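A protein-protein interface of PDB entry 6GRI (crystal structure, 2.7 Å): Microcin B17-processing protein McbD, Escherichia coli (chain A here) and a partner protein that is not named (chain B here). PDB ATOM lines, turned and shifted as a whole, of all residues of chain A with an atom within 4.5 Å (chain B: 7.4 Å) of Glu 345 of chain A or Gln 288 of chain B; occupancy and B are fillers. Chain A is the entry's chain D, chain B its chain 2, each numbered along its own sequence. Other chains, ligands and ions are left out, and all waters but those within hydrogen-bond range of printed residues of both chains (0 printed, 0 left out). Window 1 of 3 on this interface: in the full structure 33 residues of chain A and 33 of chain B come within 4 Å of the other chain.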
ATOM      1  N   PHE A  59      18.956  16.400 -10.236  1.00  0.00           N
ATOM      2  CA  PHE A  59      18.764  16.086  -8.811  1.00  0.00           C
ATOM      3  C   PHE A  59      18.498  14.576  -8.587  1.00  0.00           C
ATOM      4  O   PHE A  59      19.067  13.976  -7.671  1.00  0.00           O
ATOM      5  CB  PHE A  59      17.623  16.927  -8.199  1.00  0.00           C
ATOM      6  CG  PHE A  59      18.073  18.206  -7.541  1.00  0.00           C
ATOM      7  CD1 PHE A  59      18.534  18.199  -6.233  1.00  0.00           C
ATOM      8  CD2 PHE A  59      18.001  19.417  -8.207  1.00  0.00           C
ATOM      9  CE1 PHE A  59      18.928  19.368  -5.605  1.00  0.00           C
ATOM     10  CE2 PHE A  59      18.398  20.591  -7.597  1.00  0.00           C
ATOM     11  CZ  PHE A  59      18.864  20.571  -6.293  1.00  0.00           C
ATOM     12  N   HIS A  63      21.147  11.916  -6.527  1.00  0.00           N
ATOM     13  CA  HIS A  63      20.724  11.210  -5.314  1.00  0.00           C
ATOM     14  C   HIS A  63      20.953   9.692  -5.379  1.00  0.00           C
ATOM     15  O   HIS A  63      21.591   9.123  -4.489  1.00  0.00           O
ATOM     16  CB  HIS A  63      19.257  11.524  -4.990  1.00  0.00           C
ATOM     17  CG  HIS A  63      18.736  10.804  -3.785  1.00  0.00           C
ATOM     18  ND1 HIS A  63      19.169  11.082  -2.506  1.00  0.00           N
ATOM     19  CD2 HIS A  63      17.825   9.809  -3.667  1.00  0.00           C
ATOM     20  CE1 HIS A  63      18.542  10.290  -1.654  1.00  0.00           C
ATOM     21  NE2 HIS A  63      17.716   9.514  -2.331  1.00  0.00           N
ATOM     22  N   GLU A  67      24.012   9.823  -2.831  1.00  0.00           N
ATOM     23  CA  GLU A  67      23.481  10.317  -1.543  1.00  0.00           C
ATOM     24  C   GLU A  67      22.610   9.311  -0.763  1.00  0.00           C
ATOM     25  O   GLU A  67      21.837   9.715   0.119  1.00  0.00           O
ATOM     26  CB  GLU A  67      22.662  11.599  -1.796  1.00  0.00           C
ATOM     27  CG  GLU A  67      23.467  12.750  -2.391  1.00  0.00           C
ATOM     28  CD  GLU A  67      22.670  13.654  -3.325  1.00  0.00           C
ATOM     29  OE1 GLU A  67      21.440  13.819  -3.128  1.00  0.00           O
ATOM     30  OE2 GLU A  67      23.295  14.218  -4.253  1.00  0.00           O
ATOM     31  N   ALA A 343      13.080   9.621   0.358  1.00  0.00           N
ATOM     32  CA  ALA A 343      14.100  10.415   1.030  1.00  0.00           C
ATOM     33  C   ALA A 343      13.725  11.886   0.871  1.00  0.00           C
ATOM     34  O   ALA A 343      12.904  12.245   0.023  1.00  0.00           O
ATOM     35  CB  ALA A 343      15.468  10.129   0.434  1.00  0.00           C
ATOM     36  N   ARG A 344      14.306  12.741   1.696  1.00  0.00           N
ATOM     37  CA  ARG A 344      14.062  14.171   1.576  1.00  0.00           C
ATOM     38  C   ARG A 344      15.270  15.017   1.969  1.00  0.00           C
ATOM     39  O   ARG A 344      16.201  14.531   2.593  1.00  0.00           O
ATOM     40  CB  ARG A 344      12.800  14.564   2.344  1.00  0.00           C
ATOM     41  CG  ARG A 344      12.856  14.444   3.857  1.00  0.00           C
ATOM     42  CD  ARG A 344      12.780  13.008   4.338  1.00  0.00           C
ATOM     43  NE  ARG A 344      12.390  12.920   5.744  1.00  0.00           N
ATOM     44  CZ  ARG A 344      12.529  11.838   6.504  1.00  0.00           C
ATOM     45  NH1 ARG A 344      13.040  10.710   6.010  1.00  0.00           N
ATOM     46  NH2 ARG A 344      12.142  11.879   7.776  1.00  0.00           N
ATOM     47  N   GLU A 345      15.255  16.274   1.532  1.00  0.00           N
ATOM     48  CA  GLU A 345      16.308  17.257   1.808  1.00  0.00           C
ATOM     49  C   GLU A 345      15.605  18.581   2.040  1.00  0.00           C
ATOM     50  O   GLU A 345      14.504  18.783   1.533  1.00  0.00           O
ATOM     51  CB  GLU A 345      17.265  17.403   0.613  1.00  0.00           C
ATOM     52  CG  GLU A 345      18.297  16.294   0.442  1.00  0.00           C
ATOM     53  CD  GLU A 345      18.925  16.283  -0.950  1.00  0.00           C
ATOM     54  OE1 GLU A 345      18.573  17.156  -1.774  1.00  0.00           O
ATOM     55  OE2 GLU A 345      19.763  15.397  -1.231  1.00  0.00           O
ATOM     56  N   ARG A 346      16.231  19.476   2.801  1.00  0.00           N
ATOM     57  CA  ARG A 346      15.730  20.830   2.975  1.00  0.00           C
ATOM     58  C   ARG A 346      16.349  21.731   1.904  1.00  0.00           C
ATOM     59  O   ARG A 346      17.568  21.732   1.712  1.00  0.00           O
ATOM     60  CB  ARG A 346      16.068  21.327   4.373  1.00  0.00           C
ATOM     61  CG  ARG A 346      15.462  22.673   4.710  1.00  0.00           C
ATOM     62  CD  ARG A 346      16.052  23.218   5.994  1.00  0.00           C
ATOM     63  NE  ARG A 346      15.546  24.553   6.291  1.00  0.00           N
ATOM     64  CZ  ARG A 346      15.938  25.306   7.316  1.00  0.00           C
ATOM     65  NH1 ARG A 346      16.861  24.875   8.176  1.00  0.00           N
ATOM     66  NH2 ARG A 346      15.397  26.507   7.481  1.00  0.00           N
ATOM     67  N   VAL A 347      15.503  22.477   1.200  1.00  0.00           N
ATOM     68  CA  VAL A 347      15.949  23.524   0.283  1.00  0.00           C
ATOM     69  C   VAL A 347      15.224  24.807   0.663  1.00  0.00           C
ATOM     70  O   VAL A 347      14.019  24.920   0.450  1.00  0.00           O
ATOM     71  CB  VAL A 347      15.672  23.170  -1.181  1.00  0.00           C
ATOM     72  CG1 VAL A 347      16.158  24.285  -2.094  1.00  0.00           C
ATOM     73  CG2 VAL A 347      16.352  21.855  -1.541  1.00  0.00           C
ATOM     74  N   SER A 350      11.654  24.686   2.261  1.00  0.00           N
ATOM     75  CA  SER A 350      10.852  23.693   1.572  1.00  0.00           C
ATOM     76  C   SER A 350      11.503  22.351   1.771  1.00  0.00           C
ATOM     77  O   SER A 350      12.690  22.277   2.063  1.00  0.00           O
ATOM     78  CB  SER A 350      10.803  23.977   0.060  1.00  0.00           C
ATOM     79  OG  SER A 350      10.402  25.311  -0.226  1.00  0.00           O
ATOM     80  N   LEU A 351      10.708  21.298   1.614  1.00  0.00           N
ATOM     81  CA  LEU A 351      11.214  19.939   1.454  1.00  0.00           C
ATOM     82  C   LEU A 351      11.078  19.545  -0.004  1.00  0.00           C
ATOM     83  O   LEU A 351      10.082  19.862  -0.653  1.00  0.00           O
ATOM     84  CB  LEU A 351      10.455  18.953   2.339  1.00  0.00           C
ATOM     85  CG  LEU A 351      10.782  19.089   3.823  1.00  0.00           C
ATOM     86  CD1 LEU A 351       9.731  18.397   4.671  1.00  0.00           C
ATOM     87  CD2 LEU A 351      12.168  18.533   4.122  1.00  0.00           C
ATOM     88  N   VAL A 352      12.114  18.888  -0.507  1.00  0.00           N
ATOM     89  CA  VAL A 352      12.114  18.249  -1.819  1.00  0.00           C
ATOM     90  C   VAL A 352      12.310  16.759  -1.558  1.00  0.00           C
ATOM     91  O   VAL A 352      12.848  16.366  -0.520  1.00  0.00           O
ATOM     92  CB  VAL A 352      13.196  18.811  -2.769  1.00  0.00           C
ATOM     93  CG1 VAL A 352      12.912  20.268  -3.073  1.00  0.00           C
ATOM     94  CG2 VAL A 352      14.610  18.659  -2.206  1.00  0.00           C
ATOM     95  N   TYR A 354      12.723  12.541  -2.968  1.00  0.00           N
ATOM     96  CA  TYR A 354      13.149  11.477  -3.880  1.00  0.00           C
ATOM     97  C   TYR A 354      12.330  10.234  -3.544  1.00  0.00           C
ATOM     98  O   TYR A 354      12.088   9.957  -2.362  1.00  0.00           O
ATOM     99  CB  TYR A 354      14.646  11.184  -3.713  1.00  0.00           C
ATOM    100  CG  TYR A 354      15.513  12.422  -3.750  1.00  0.00           C
ATOM    101  CD1 TYR A 354      15.739  13.168  -2.598  1.00  0.00           C
ATOM    102  CD2 TYR A 354      16.090  12.858  -4.939  1.00  0.00           C
ATOM    103  CE1 TYR A 354      16.521  14.303  -2.624  1.00  0.00           C
ATOM    104  CE2 TYR A 354      16.870  13.997  -4.984  1.00  0.00           C
ATOM    105  CZ  TYR A 354      17.086  14.719  -3.825  1.00  0.00           C
ATOM    106  OH  TYR A 354      17.876  15.848  -3.859  1.00  0.00           O
ATOM    107  N   TYR B  32      10.941  16.408   8.263  1.00  0.00           N
ATOM    108  CA  TYR B  32      12.342  16.476   7.856  1.00  0.00           C
ATOM    109  C   TYR B  32      13.196  15.455   8.587  1.00  0.00           C
ATOM    110  O   TYR B  32      14.167  14.952   8.028  1.00  0.00           O
ATOM    111  CB  TYR B  32      12.901  17.885   8.117  1.00  0.00           C
ATOM    112  CG  TYR B  32      14.326  18.088   7.643  1.00  0.00           C
ATOM    113  CD1 TYR B  32      15.288  18.675   8.470  1.00  0.00           C
ATOM    114  CD2 TYR B  32      14.722  17.676   6.360  1.00  0.00           C
ATOM    115  CE1 TYR B  32      16.593  18.860   8.027  1.00  0.00           C
ATOM    116  CE2 TYR B  32      16.019  17.855   5.916  1.00  0.00           C
ATOM    117  CZ  TYR B  32      16.948  18.446   6.750  1.00  0.00           C
ATOM    118  OH  TYR B  32      18.221  18.617   6.290  1.00  0.00           O
ATOM    119  N   CYS B 195      28.980  19.219   5.067  1.00  0.00           N
ATOM    120  CA  CYS B 195      27.976  19.232   4.011  1.00  0.00           C
ATOM    121  C   CYS B 195      28.531  19.976   2.770  1.00  0.00           C
ATOM    122  O   CYS B 195      28.386  19.498   1.638  1.00  0.00           O
ATOM    123  CB  CYS B 195      26.665  19.874   4.494  1.00  0.00           C
ATOM    124  SG  CYS B 195      25.714  18.950   5.732  1.00  0.00           S
ATOM    125  N   ARG B 199      29.345  17.946  -0.965  1.00  0.00           N
ATOM    126  CA  ARG B 199      28.619  18.330  -2.187  1.00  0.00           C
ATOM    127  C   ARG B 199      29.557  18.793  -3.291  1.00  0.00           C
ATOM    128  O   ARG B 199      29.279  18.584  -4.480  1.00  0.00           O
ATOM    129  CB  ARG B 199      27.550  19.396  -1.906  1.00  0.00           C
ATOM    130  CG  ARG B 199      26.370  18.847  -1.116  1.00  0.00           C
ATOM    131  CD  ARG B 199      25.012  19.410  -1.505  1.00  0.00           C
ATOM    132  NE  ARG B 199      23.920  18.504  -1.120  1.00  0.00           N
ATOM    133  CZ  ARG B 199      23.500  17.442  -1.820  1.00  0.00           C
ATOM    134  NH1 ARG B 199      24.090  17.066  -2.954  1.00  0.00           N
ATOM    135  NH2 ARG B 199      22.478  16.734  -1.364  1.00  0.00           N
ATOM    136  N   ILE B 285      22.703  23.384   0.702  1.00  0.00           N
ATOM    137  CA  ILE B 285      21.757  22.324   1.071  1.00  0.00           C
ATOM    138  C   ILE B 285      22.546  21.250   1.794  1.00  0.00           C
ATOM    139  O   ILE B 285      23.733  21.072   1.514  1.00  0.00           O
ATOM    140  CB  ILE B 285      21.043  21.731  -0.167  1.00  0.00           C
ATOM    141  CG1 ILE B 285      22.052  21.189  -1.180  1.00  0.00           C
ATOM    142  CG2 ILE B 285      20.151  22.786  -0.814  1.00  0.00           C
ATOM    143  CD1 ILE B 285      21.501  20.970  -2.574  1.00  0.00           C
ATOM    144  N   HIS B 286      21.897  20.527   2.709  1.00  0.00           N
ATOM    145  CA  HIS B 286      22.606  19.512   3.530  1.00  0.00           C
ATOM    146  C   HIS B 286      23.143  18.348   2.683  1.00  0.00           C
ATOM    147  O   HIS B 286      22.756  18.177   1.519  1.00  0.00           O
ATOM    148  CB  HIS B 286      21.710  18.905   4.619  1.00  0.00           C
ATOM    149  CG  HIS B 286      21.112  19.900   5.561  1.00  0.00           C
ATOM    150  ND1 HIS B 286      20.053  20.712   5.213  1.00  0.00           N
ATOM    151  CD2 HIS B 286      21.401  20.190   6.851  1.00  0.00           C
ATOM    152  CE1 HIS B 286      19.724  21.470   6.244  1.00  0.00           C
ATOM    153  NE2 HIS B 286      20.526  21.173   7.251  1.00  0.00           N
ATOM    154  N   TRP B 287      24.051  17.570   3.265  1.00  0.00           N
ATOM    155  CA  TRP B 287      24.261  16.208   2.797  1.00  0.00           C
ATOM    156  C   TRP B 287      23.454  15.321   3.730  1.00  0.00           C
ATOM    157  O   TRP B 287      23.496  15.492   4.949  1.00  0.00           O
ATOM    158  CB  TRP B 287      25.746  15.811   2.747  1.00  0.00           C
ATOM    159  CG  TRP B 287      26.122  15.232   1.404  1.00  0.00           C
ATOM    160  CD1 TRP B 287      25.790  15.744   0.178  1.00  0.00           C
ATOM    161  CD2 TRP B 287      26.889  14.054   1.145  1.00  0.00           C
ATOM    162  NE1 TRP B 287      26.301  14.964  -0.833  1.00  0.00           N
ATOM    163  CE2 TRP B 287      26.981  13.915  -0.271  1.00  0.00           C
ATOM    164  CE3 TRP B 287      27.514  13.111   1.957  1.00  0.00           C
ATOM    165  CZ2 TRP B 287      27.671  12.857  -0.885  1.00  0.00           C
ATOM    166  CZ3 TRP B 287      28.204  12.052   1.345  1.00  0.00           C
ATOM    167  CH2 TRP B 287      28.276  11.940  -0.067  1.00  0.00           C
ATOM    168  N   GLN B 288      22.684  14.405   3.149  1.00  0.00           N
ATOM    169  CA  GLN B 288      21.897  13.454   3.928  1.00  0.00           C
ATOM    170  C   GLN B 288      22.804  12.561   4.781  1.00  0.00           C
ATOM    171  O   GLN B 288      22.479  12.278   5.927  1.00  0.00           O
ATOM    172  CB  GLN B 288      21.038  12.585   3.013  1.00  0.00           C
ATOM    173  CG  GLN B 288      19.927  13.328   2.289  1.00  0.00           C
ATOM    174  CD  GLN B 288      19.177  12.439   1.307  1.00  0.00           C
ATOM    175  OE1 GLN B 288      18.933  12.834   0.163  1.00  0.00           O
ATOM    176  NE2 GLN B 288      18.810  11.228   1.748  1.00  0.00           N
ATOM    177  N   ALA B 289      23.944  12.143   4.225  1.00  0.00           N
ATOM    178  CA  ALA B 289      24.882  11.255   4.930  1.00  0.00           C
ATOM    179  C   ALA B 289      25.549  11.900   6.152  1.00  0.00           C
ATOM    180  O   ALA B 289      25.960  11.195   7.075  1.00  0.00           O
ATOM    181  CB  ALA B 289      25.943  10.721   3.970  1.00  0.00           C
ATOM    182  N   CYS B 290      25.650  13.227   6.151  1.00  0.00           N
ATOM    183  CA  CYS B 290      26.266  13.972   7.250  1.00  0.00           C
ATOM    184  C   CYS B 290      25.436  13.927   8.535  1.00  0.00           C
ATOM    185  O   CYS B 290      24.206  13.956   8.494  1.00  0.00           O
ATOM    186  CB  CYS B 290      26.466  15.435   6.830  1.00  0.00           C
ATOM    187  SG  CYS B 290      27.543  16.391   7.917  1.00  0.00           S
ATOM    188  N   SER B 291      26.120  13.884   9.673  1.00  0.00           N
ATOM    189  CA  SER B 291      25.463  13.850  10.990  1.00  0.00           C
ATOM    190  C   SER B 291      24.748  15.144  11.399  1.00  0.00           C
ATOM    191  O   SER B 291      23.620  15.089  11.875  1.00  0.00           O
ATOM    192  CB  SER B 291      26.484  13.486  12.074  1.00  0.00           C
ATOM    193  OG  SER B 291      27.677  14.239  11.942  1.00  0.00           O
ATOM    194  N   CYS B 292      25.409  16.283  11.179  1.00  0.00           N
ATOM    195  CA  CYS B 292      25.104  17.593  11.817  1.00  0.00           C
ATOM    196  C   CYS B 292      23.646  17.935  12.197  1.00  0.00           C
ATOM    197  O   CYS B 292      22.676  17.434  11.624  1.00  0.00           O
ATOM    198  CB  CYS B 292      25.705  18.736  10.969  1.00  0.00           C
ATOM    199  SG  CYS B 292      25.130  18.893   9.253  1.00  0.00           S
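The side-chain carboxylate (OE2) of Glu 345 of chain A lies close to the side-chain amide oxygen (OE1) of Gln 288 of chain B, 3.0 Å away. The guanidinium group of Arg 199 of chain B is in salt-bridge range of the side-chain carboxylate of Glu 67 of chain A (3.2 Å). The side-chain amide oxygen (OE1) of Gln 288 of chain B lies close to a ring nitrogen (ND1) of His 63 of chain A, at 3.2 Å. The side-chain carboxylate (OE2) of Glu 345 of chain A is in salt-bridge range of the guanidinium group (NH2) of Arg 199 of chain B.
O of His 286 of chain B lies within hydrogen-bond range of NE of Arg 199 of chain B (2.9 Å). The backbone NH of Val 352 of chain A sits at hydrogen-bond distance from the backbone carbonyl oxygen of Glu 345 of chain A (3.1 Å). The backbone NH (N) of Trp 287 of chain B sits close to the side-chain sulfur (SG) of Cys 195 of chain B. The backbone carbonyl oxygen (O) of Tyr 354 of chain A lies within hydrogen-bond range of the backbone NH (N) of Ala 343 of chain A (2.9 Å). The side-chain carboxylate of Glu 345 of chain A sits at hydrogen-bond distance from the side-chain hydroxyl of Tyr 354 of chain A. ND1 of His 286 of chain B lies within hydrogen-bond range of OH of Tyr 32 of chain B (3.0 Å).
CG of Glu 67 of chain A touches NE1 of Trp 287 of chain B, at 3.9 Å. Glu 67 of chain A touches Gln 288 of chain B. Ala 343 of chain A touches Gln 288 of chain B (CB to NE2, 3.8 Å). NE of Arg 344 of chain A touches O of Tyr 32 of chain B, at 3.5 Å. Arg 344 of chain A touches Gln 288 of chain B. Glu 345 of chain A touches Tyr 32 of chain B (C to CE2, 3.97 Å). Tyr 32 of chain B touches Arg 346 of chain A. Arg 346 of chain A touches Ile 285 of chain B. Tyr 32 of chain B touches Leu 351 of chain A (CD2 to CD2, 3.5 Å). Gln 288 of chain B touches Tyr 354 of chain A (OE1 to CE1, 3.97 Å).
Of the printed residues of chain B, Glu 345 of chain A touches Tyr 32 (3.97 Å), Arg 199 (3.0 Å) and Gln 288 (3.0 Å). Of the printed residues of chain A, Gln 288 of chain B touches His 63 (3.2 Å), Glu 67 (3.8 Å), Ala 343 (3.8 Å), Arg 344 (3.9 Å), Glu 345 (3.0 Å) and Tyr 354 (3.97 Å). Of the printed residues of chain B, Glu 67 of chain A touches Arg 199, Trp 287 and Gln 288. Of the printed residues of chain A, Ile 285 of chain B touches Arg 346 (3.8 Å) and Val 347 (3.98 Å). Printed residues of chain B within 4 Å of Arg 344 of chain A: Tyr 32 (3.5 Å) and Gln 288 (3.9 Å). Of the printed residues of chain B, Arg 346 of chain A touches Tyr 32 (3.5 Å) and Ile 285 (3.8 Å). The nearest printed residue of chain B that does not touch Glu 345 of chain A is Ile 285 of chain B (4.9 Å).
Hydrophobic or aromatic side chains of chain A that line the printed part of chain B: His 63, Ala 343, Val 347, Leu 351 and Tyr 354. Hydrophobic or aromatic side chains of chain B that line the printed part of chain A: Tyr 32, Ile 285 and Trp 287. Among the printed residues, Asp or Glu carboxylates within 4 Å of a Lys or Arg side-chain nitrogen of the other chain: Glu 67 of chain A with Arg 199 of chain B and Glu 345 of chain A with Arg 199 of chain B.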
